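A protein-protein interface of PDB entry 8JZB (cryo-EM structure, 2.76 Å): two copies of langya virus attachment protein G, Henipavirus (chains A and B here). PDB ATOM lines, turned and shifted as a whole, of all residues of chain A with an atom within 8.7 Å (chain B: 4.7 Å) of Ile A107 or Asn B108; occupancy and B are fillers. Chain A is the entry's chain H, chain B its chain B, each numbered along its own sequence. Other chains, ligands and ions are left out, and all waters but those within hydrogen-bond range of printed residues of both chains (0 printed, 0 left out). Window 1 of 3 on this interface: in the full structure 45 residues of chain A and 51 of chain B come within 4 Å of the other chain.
ND2 of Asn B108 sits close to NZ of Lys A103, 3.4 Å away.
Lys A103 touches Val B104. Lys A103 touches Ser B105. Val B104 touches Ile A107 (O to CD1, 3.9 Å). Ile A107 touches Ile B107. Asn B108 touches Ile A107 (CA to CG1, 3.9 Å).
Ile A107 touches just these residues of chain B: Val B104 (3.9 Å), Ile B107 (3.9 Å) and Asn B108 (3.9 Å). Of chain A, only Lys A103 (3.4 Å) and Ile A107 (3.9 Å) come within 4 Å of Asn B108. Of the printed residues of chain A, Ile B107 touches Ile A107 (3.9 Å). Printed residues of chain B within 4 Å of Lys A103: Val B104 (3.96 Å), Ser B105 (3.7 Å) and Asn B108 (3.4 Å). Printed residues of chain A within 4 Å of Val B104: Lys A103 and Ile A107. Printed residues of chain A within 4 Å of Ser B105: Lys A103 (3.7 Å). The nearest residue of chain B that does not touch Ile A107 is Val B111 (4.2 Å).
Of the 19 printed residues of chain A, 2 touch a printed residue of chain B. Hydrophobic or aromatic side chains of chain A within 4 Å of the printed part of chain B: Ile A107. Of the 11 printed residues of chain B, 4 touch a printed residue of chain A. Printed residues of chain B that touch a printed residue of chain A: Val B104, Ser B105, Ile B107 and Asn B108.
Ile A107 touches Val B104, but with the chains exchanged Val A104 does not touch Ile B107 (7.9 Å). Ile A107 touches its own counterpart, Ile B107. Ile A107 touches Asn B108, but with the chains exchanged Asn A108 does not touch Ile B107 (7.7 Å). 10 positions are printed for both chains.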
ATOM      1  N   GLU A  99      -1.226  -2.866  -5.915  1.00  0.00           N
ATOM      2  CA  GLU A  99       0.189  -2.740  -5.594  1.00  0.00           C
ATOM      3  C   GLU A  99       0.799  -1.436  -6.084  1.00  0.00           C
ATOM      4  O   GLU A  99       1.513  -0.770  -5.326  1.00  0.00           O
ATOM      5  CB  GLU A  99       0.959  -3.934  -6.178  1.00  0.00           C
ATOM      6  CG  GLU A  99       2.463  -3.856  -6.000  1.00  0.00           C
ATOM      7  CD  GLU A  99       3.133  -5.207  -6.141  1.00  0.00           C
ATOM      8  OE1 GLU A  99       2.658  -6.023  -6.957  1.00  0.00           O
ATOM      9  OE2 GLU A  99       4.135  -5.453  -5.437  1.00  0.00           O
ATOM     10  N   ILE A 100       0.539  -1.051  -7.335  1.00  0.00           N
ATOM     11  CA  ILE A 100       1.274   0.055  -7.947  1.00  0.00           C
ATOM     12  C   ILE A 100       0.893   1.383  -7.302  1.00  0.00           C
ATOM     13  O   ILE A 100       1.756   2.217  -7.005  1.00  0.00           O
ATOM     14  CB  ILE A 100       1.041   0.073  -9.469  1.00  0.00           C
ATOM     15  CG1 ILE A 100       2.027  -0.865 -10.164  1.00  0.00           C
ATOM     16  CG2 ILE A 100       1.178   1.482 -10.025  1.00  0.00           C
ATOM     17  CD1 ILE A 100       1.729  -1.085 -11.627  1.00  0.00           C
ATOM     18  N   LYS A 101      -0.403   1.605  -7.086  1.00  0.00           N
ATOM     19  CA  LYS A 101      -0.859   2.891  -6.562  1.00  0.00           C
ATOM     20  C   LYS A 101      -0.321   3.214  -5.168  1.00  0.00           C
ATOM     21  O   LYS A 101       0.148   4.351  -4.969  1.00  0.00           O
ATOM     22  CB  LYS A 101      -2.393   2.926  -6.591  1.00  0.00           C
ATOM     23  CG  LYS A 101      -3.025   4.191  -6.043  1.00  0.00           C
ATOM     24  CD  LYS A 101      -4.521   3.991  -5.853  1.00  0.00           C
ATOM     25  CE  LYS A 101      -5.194   5.230  -5.289  1.00  0.00           C
ATOM     26  NZ  LYS A 101      -5.228   6.341  -6.279  1.00  0.00           N
ATOM     27  N   PRO A 102      -0.370   2.313  -4.176  1.00  0.00           N
ATOM     28  CA  PRO A 102       0.245   2.647  -2.880  1.00  0.00           C
ATOM     29  C   PRO A 102       1.734   2.923  -2.975  1.00  0.00           C
ATOM     30  O   PRO A 102       2.241   3.804  -2.272  1.00  0.00           O
ATOM     31  CB  PRO A 102      -0.052   1.407  -2.026  1.00  0.00           C
ATOM     32  CG  PRO A 102      -1.253   0.805  -2.651  1.00  0.00           C
ATOM     33  CD  PRO A 102      -1.059   1.011  -4.117  1.00  0.00           C
ATOM     34  N   LYS A 103       2.452   2.194  -3.833  1.00  0.00           N
ATOM     35  CA  LYS A 103       3.881   2.445  -3.990  1.00  0.00           C
ATOM     36  C   LYS A 103       4.135   3.807  -4.619  1.00  0.00           C
ATOM     37  O   LYS A 103       5.086   4.502  -4.247  1.00  0.00           O
ATOM     38  CB  LYS A 103       4.521   1.335  -4.822  1.00  0.00           C
ATOM     39  CG  LYS A 103       4.395  -0.042  -4.199  1.00  0.00           C
ATOM     40  CD  LYS A 103       5.078  -1.101  -5.043  1.00  0.00           C
ATOM     41  CE  LYS A 103       6.568  -1.143  -4.772  1.00  0.00           C
ATOM     42  NZ  LYS A 103       6.861  -1.710  -3.430  1.00  0.00           N
ATOM     43  N   VAL A 104       3.295   4.208  -5.576  1.00  0.00           N
ATOM     44  CA  VAL A 104       3.425   5.535  -6.172  1.00  0.00           C
ATOM     45  C   VAL A 104       3.193   6.611  -5.120  1.00  0.00           C
ATOM     46  O   VAL A 104       3.924   7.608  -5.054  1.00  0.00           O
ATOM     47  CB  VAL A 104       2.460   5.682  -7.364  1.00  0.00           C
ATOM     48  CG1 VAL A 104       2.272   7.144  -7.725  1.00  0.00           C
ATOM     49  CG2 VAL A 104       2.976   4.901  -8.558  1.00  0.00           C
ATOM     50  N   SER A 105       2.175   6.424  -4.275  1.00  0.00           N
ATOM     51  CA  SER A 105       1.927   7.389  -3.206  1.00  0.00           C
ATOM     52  C   SER A 105       3.098   7.450  -2.230  1.00  0.00           C
ATOM     53  O   SER A 105       3.492   8.537  -1.785  1.00  0.00           O
ATOM     54  CB  SER A 105       0.632   7.038  -2.474  1.00  0.00           C
ATOM     55  OG  SER A 105       0.854   6.036  -1.497  1.00  0.00           O
ATOM     56  N   LEU A 106       3.668   6.292  -1.886  1.00  0.00           N
ATOM     57  CA  LEU A 106       4.815   6.263  -0.982  1.00  0.00           C
ATOM     58  C   LEU A 106       6.020   6.968  -1.589  1.00  0.00           C
ATOM     59  O   LEU A 106       6.740   7.692  -0.894  1.00  0.00           O
ATOM     60  CB  LEU A 106       5.167   4.819  -0.625  1.00  0.00           C
ATOM     61  CG  LEU A 106       4.250   4.099   0.362  1.00  0.00           C
ATOM     62  CD1 LEU A 106       4.768   2.699   0.640  1.00  0.00           C
ATOM     63  CD2 LEU A 106       4.120   4.888   1.651  1.00  0.00           C
ATOM     64  N   ILE A 107       6.263   6.761  -2.885  1.00  0.00           N
ATOM     65  CA  ILE A 107       7.380   7.428  -3.549  1.00  0.00           C
ATOM     66  C   ILE A 107       7.165   8.935  -3.568  1.00  0.00           C
ATOM     67  O   ILE A 107       8.103   9.714  -3.350  1.00  0.00           O
ATOM     68  CB  ILE A 107       7.578   6.862  -4.968  1.00  0.00           C
ATOM     69  CG1 ILE A 107       8.054   5.411  -4.904  1.00  0.00           C
ATOM     70  CG2 ILE A 107       8.570   7.704  -5.747  1.00  0.00           C
ATOM     71  CD1 ILE A 107       7.726   4.609  -6.138  1.00  0.00           C
ATOM     72  N   ASN A 108       5.930   9.372  -3.835  1.00  0.00           N
ATOM     73  CA  ASN A 108       5.634  10.801  -3.808  1.00  0.00           C
ATOM     74  C   ASN A 108       5.894  11.392  -2.430  1.00  0.00           C
ATOM     75  O   ASN A 108       6.501  12.464  -2.308  1.00  0.00           O
ATOM     76  CB  ASN A 108       4.187  11.047  -4.227  1.00  0.00           C
ATOM     77  CG  ASN A 108       3.892  12.513  -4.466  1.00  0.00           C
ATOM     78  OD1 ASN A 108       4.717  13.242  -5.013  1.00  0.00           O
ATOM     79  ND2 ASN A 108       2.714  12.955  -4.046  1.00  0.00           N
ATOM     80  N   THR A 109       5.451  10.701  -1.377  1.00  0.00           N
ATOM     81  CA  THR A 109       5.704  11.182  -0.023  1.00  0.00           C
ATOM     82  C   THR A 109       7.199  11.229   0.277  1.00  0.00           C
ATOM     83  O   THR A 109       7.682  12.171   0.913  1.00  0.00           O
ATOM     84  CB  THR A 109       4.985  10.297   0.995  1.00  0.00           C
ATOM     85  OG1 THR A 109       3.606  10.171   0.630  1.00  0.00           O
ATOM     86  CG2 THR A 109       5.081  10.899   2.386  1.00  0.00           C
ATOM     87  N   ALA A 110       7.943  10.217  -0.171  1.00  0.00           N
ATOM     88  CA  ALA A 110       9.376  10.169   0.100  1.00  0.00           C
ATOM     89  C   ALA A 110      10.119  11.302  -0.595  1.00  0.00           C
ATOM     90  O   ALA A 110      11.016  11.916  -0.007  1.00  0.00           O
ATOM     91  CB  ALA A 110       9.945   8.818  -0.328  1.00  0.00           C
ATOM     92  N   VAL A 111       9.769  11.594  -1.845  1.00  0.00           N
ATOM     93  CA  VAL A 111      10.522  12.590  -2.606  1.00  0.00           C
ATOM     94  C   VAL A 111      10.065  14.008  -2.288  1.00  0.00           C
ATOM     95  O   VAL A 111      10.828  14.960  -2.463  1.00  0.00           O
ATOM     96  CB  VAL A 111      10.429  12.302  -4.119  1.00  0.00           C
ATOM     97  CG1 VAL A 111      11.012  10.937  -4.442  1.00  0.00           C
ATOM     98  CG2 VAL A 111       8.997  12.430  -4.612  1.00  0.00           C
ATOM     99  N   SER A 112       8.826  14.186  -1.824  1.00  0.00           N
ATOM    100  CA  SER A 112       8.314  15.540  -1.643  1.00  0.00           C
ATOM    101  C   SER A 112       8.522  16.046  -0.219  1.00  0.00           C
ATOM    102  O   SER A 112       8.597  17.260   0.004  1.00  0.00           O
ATOM    103  CB  SER A 112       6.834  15.593  -2.017  1.00  0.00           C
ATOM    104  OG  SER A 112       6.651  15.331  -3.397  1.00  0.00           O
ATOM    105  N   VAL A 113       8.615  15.144   0.757  1.00  0.00           N
ATOM    106  CA  VAL A 113       8.612  15.558   2.158  1.00  0.00           C
ATOM    107  C   VAL A 113       9.882  15.129   2.885  1.00  0.00           C
ATOM    108  O   VAL A 113      10.617  15.970   3.412  1.00  0.00           O
ATOM    109  CB  VAL A 113       7.368  15.015   2.884  1.00  0.00           C
ATOM    110  CG1 VAL A 113       7.252  15.633   4.263  1.00  0.00           C
ATOM    111  CG2 VAL A 113       6.114  15.290   2.073  1.00  0.00           C
ATOM    112  N   SER A 114      10.140  13.819   2.931  1.00  0.00           N
ATOM    113  CA  SER A 114      11.152  13.291   3.845  1.00  0.00           C
ATOM    114  C   SER A 114      12.562  13.739   3.471  1.00  0.00           C
ATOM    115  O   SER A 114      13.310  14.229   4.327  1.00  0.00           O
ATOM    116  CB  SER A 114      11.073  11.766   3.880  1.00  0.00           C
ATOM    117  OG  SER A 114       9.732  11.329   4.005  1.00  0.00           O
ATOM    118  N   ILE A 115      12.946  13.563   2.211  1.00  0.00           N
ATOM    119  CA  ILE A 115      14.302  13.865   1.752  1.00  0.00           C
ATOM    120  C   ILE A 115      14.610  15.356   1.896  1.00  0.00           C
ATOM    121  O   ILE A 115      15.705  15.702   2.369  1.00  0.00           O
ATOM    122  CB  ILE A 115      14.514  13.372   0.312  1.00  0.00           C
ATOM    123  CG1 ILE A 115      14.562  11.843   0.280  1.00  0.00           C
ATOM    124  CG2 ILE A 115      15.787  13.948  -0.275  1.00  0.00           C
ATOM    125  CD1 ILE A 115      14.694  11.266  -1.106  1.00  0.00           C
ATOM    126  N   LEU A 271      -0.280  16.455  -1.317  1.00  0.00           N
ATOM    127  CA  LEU A 271      -0.321  15.027  -1.038  1.00  0.00           C
ATOM    128  C   LEU A 271      -1.606  14.363  -1.509  1.00  0.00           C
ATOM    129  O   LEU A 271      -1.585  13.169  -1.824  1.00  0.00           O
ATOM    130  CB  LEU A 271      -0.144  14.767   0.461  1.00  0.00           C
ATOM    131  CG  LEU A 271       1.053  15.422   1.149  1.00  0.00           C
ATOM    132  CD1 LEU A 271       0.894  15.351   2.656  1.00  0.00           C
ATOM    133  CD2 LEU A 271       2.347  14.760   0.712  1.00  0.00           C
ATOM    134  N   ASP A 325      -2.963   9.859   3.535  1.00  0.00           N
ATOM    135  CA  ASP A 325      -2.749   8.453   3.196  1.00  0.00           C
ATOM    136  C   ASP A 325      -4.001   7.614   3.444  1.00  0.00           C
ATOM    137  O   ASP A 325      -3.930   6.435   3.798  1.00  0.00           O
ATOM    138  CB  ASP A 325      -1.554   7.888   3.968  1.00  0.00           C
ATOM    139  CG  ASP A 325      -0.362   7.603   3.075  1.00  0.00           C
ATOM    140  OD1 ASP A 325      -0.516   7.659   1.838  1.00  0.00           O
ATOM    141  OD2 ASP A 325       0.730   7.326   3.615  1.00  0.00           O
ATOM    142  N   VAL B 104       9.191   0.156 -10.613  1.00  0.00           N
ATOM    143  CA  VAL B 104       8.544   0.898  -9.533  1.00  0.00           C
ATOM    144  C   VAL B 104       9.033   0.396  -8.181  1.00  0.00           C
ATOM    145  O   VAL B 104       9.300   1.186  -7.266  1.00  0.00           O
ATOM    146  CB  VAL B 104       7.012   0.799  -9.661  1.00  0.00           C
ATOM    147  CG1 VAL B 104       6.340   1.063  -8.327  1.00  0.00           C
ATOM    148  CG2 VAL B 104       6.508   1.771 -10.712  1.00  0.00           C
ATOM    149  N   SER B 105       9.167  -0.925  -8.036  1.00  0.00           N
ATOM    150  CA  SER B 105       9.717  -1.472  -6.799  1.00  0.00           C
ATOM    151  C   SER B 105      11.155  -1.015  -6.572  1.00  0.00           C
ATOM    152  O   SER B 105      11.532  -0.690  -5.439  1.00  0.00           O
ATOM    153  CB  SER B 105       9.642  -2.996  -6.819  1.00  0.00           C
ATOM    154  OG  SER B 105       8.316  -3.436  -7.054  1.00  0.00           O
ATOM    155  N   LEU B 106      11.965  -0.987  -7.633  1.00  0.00           N
ATOM    156  CA  LEU B 106      13.339  -0.506  -7.512  1.00  0.00           C
ATOM    157  C   LEU B 106      13.380   0.955  -7.084  1.00  0.00           C
ATOM    158  O   LEU B 106      14.195   1.336  -6.235  1.00  0.00           O
ATOM    159  CB  LEU B 106      14.077  -0.693  -8.836  1.00  0.00           C
ATOM    160  CG  LEU B 106      15.149  -1.780  -8.893  1.00  0.00           C
ATOM    161  CD1 LEU B 106      14.519  -3.161  -8.866  1.00  0.00           C
ATOM    162  CD2 LEU B 106      16.006  -1.608 -10.134  1.00  0.00           C
ATOM    163  N   ILE B 107      12.512   1.789  -7.664  1.00  0.00           N
ATOM    164  CA  ILE B 107      12.459   3.196  -7.283  1.00  0.00           C
ATOM    165  C   ILE B 107      12.054   3.343  -5.826  1.00  0.00           C
ATOM    166  O   ILE B 107      12.636   4.151  -5.091  1.00  0.00           O
ATOM    167  CB  ILE B 107      11.502   3.973  -8.212  1.00  0.00           C
ATOM    168  CG1 ILE B 107      12.093   4.090  -9.617  1.00  0.00           C
ATOM    169  CG2 ILE B 107      11.209   5.353  -7.652  1.00  0.00           C
ATOM    170  CD1 ILE B 107      11.055   4.095 -10.714  1.00  0.00           C
ATOM    171  N   ASN B 108      11.054   2.578  -5.383  1.00  0.00           N
ATOM    172  CA  ASN B 108      10.644   2.633  -3.983  1.00  0.00           C
ATOM    173  C   ASN B 108      11.792   2.259  -3.058  1.00  0.00           C
ATOM    174  O   ASN B 108      12.060   2.958  -2.072  1.00  0.00           O
ATOM    175  CB  ASN B 108       9.450   1.709  -3.747  1.00  0.00           C
ATOM    176  CG  ASN B 108       8.927   1.786  -2.328  1.00  0.00           C
ATOM    177  OD1 ASN B 108       8.824   2.867  -1.751  1.00  0.00           O
ATOM    178  ND2 ASN B 108       8.602   0.635  -1.755  1.00  0.00           N
ATOM    179  N   THR B 109      12.491   1.166  -3.369  1.00  0.00           N
ATOM    180  CA  THR B 109      13.617   0.749  -2.540  1.00  0.00           C
ATOM    181  C   THR B 109      14.711   1.809  -2.513  1.00  0.00           C
ATOM    182  O   THR B 109      15.271   2.096  -1.449  1.00  0.00           O
ATOM    183  CB  THR B 109      14.170  -0.585  -3.044  1.00  0.00           C
ATOM    184  OG1 THR B 109      13.375  -1.659  -2.530  1.00  0.00           O
ATOM    185  CG2 THR B 109      15.612  -0.779  -2.602  1.00  0.00           C
ATOM    186  N   ALA B 110      15.012   2.415  -3.660  1.00  0.00           N
ATOM    187  CA  ALA B 110      16.096   3.386  -3.725  1.00  0.00           C
ATOM    188  C   ALA B 110      15.753   4.684  -3.002  1.00  0.00           C
ATOM    189  O   ALA B 110      16.631   5.299  -2.388  1.00  0.00           O
ATOM    190  CB  ALA B 110      16.459   3.667  -5.180  1.00  0.00           C
ATOM    191  N   VAL B 111      14.494   5.125  -3.059  1.00  0.00           N
ATOM    192  CA  VAL B 111      14.152   6.405  -2.442  1.00  0.00           C
ATOM    193  C   VAL B 111      13.852   6.230  -0.958  1.00  0.00           C
ATOM    194  O   VAL B 111      13.936   7.187  -0.181  1.00  0.00           O
ATOM    195  CB  VAL B 111      12.973   7.076  -3.172  1.00  0.00           C
ATOM    196  CG1 VAL B 111      13.305   7.305  -4.636  1.00  0.00           C
ATOM    197  CG2 VAL B 111      11.696   6.268  -3.003  1.00  0.00           C
ATOM    198  N   SER B 112      13.494   5.017  -0.538  1.00  0.00           N
ATOM    199  CA  SER B 112      13.105   4.803   0.849  1.00  0.00           C
ATOM    200  C   SER B 112      14.211   4.217   1.715  1.00  0.00           C
ATOM    201  O   SER B 112      14.097   4.262   2.943  1.00  0.00           O
ATOM    202  CB  SER B 112      11.878   3.889   0.914  1.00  0.00           C
ATOM    203  OG  SER B 112      10.682   4.644   0.976  1.00  0.00           O
ATOM    204  N   VAL B 113      15.273   3.673   1.123  1.00  0.00           N
ATOM    205  CA  VAL B 113      16.304   2.995   1.901  1.00  0.00           C
ATOM    206  C   VAL B 113      17.682   3.585   1.632  1.00  0.00           C
ATOM    207  O   VAL B 113      18.397   3.967   2.564  1.00  0.00           O
ATOM    208  CB  VAL B 113      16.298   1.482   1.616  1.00  0.00           C
ATOM    209  CG1 VAL B 113      17.474   0.810   2.301  1.00  0.00           C
ATOM    210  CG2 VAL B 113      14.990   0.859   2.068  1.00  0.00           C
ATOM    211  N   PRO B 270       8.207   0.529   4.748  1.00  0.00           N
ATOM    212  CA  PRO B 270       7.589  -0.713   4.261  1.00  0.00           C
ATOM    213  C   PRO B 270       8.144  -1.099   2.897  1.00  0.00           C
ATOM    214  O   PRO B 270       8.316  -0.252   2.019  1.00  0.00           O
ATOM    215  CB  PRO B 270       6.099  -0.361   4.178  1.00  0.00           C
ATOM    216  CG  PRO B 270       5.936   0.816   5.085  1.00  0.00           C
ATOM    217  CD  PRO B 270       7.208   1.590   4.950  1.00  0.00           C
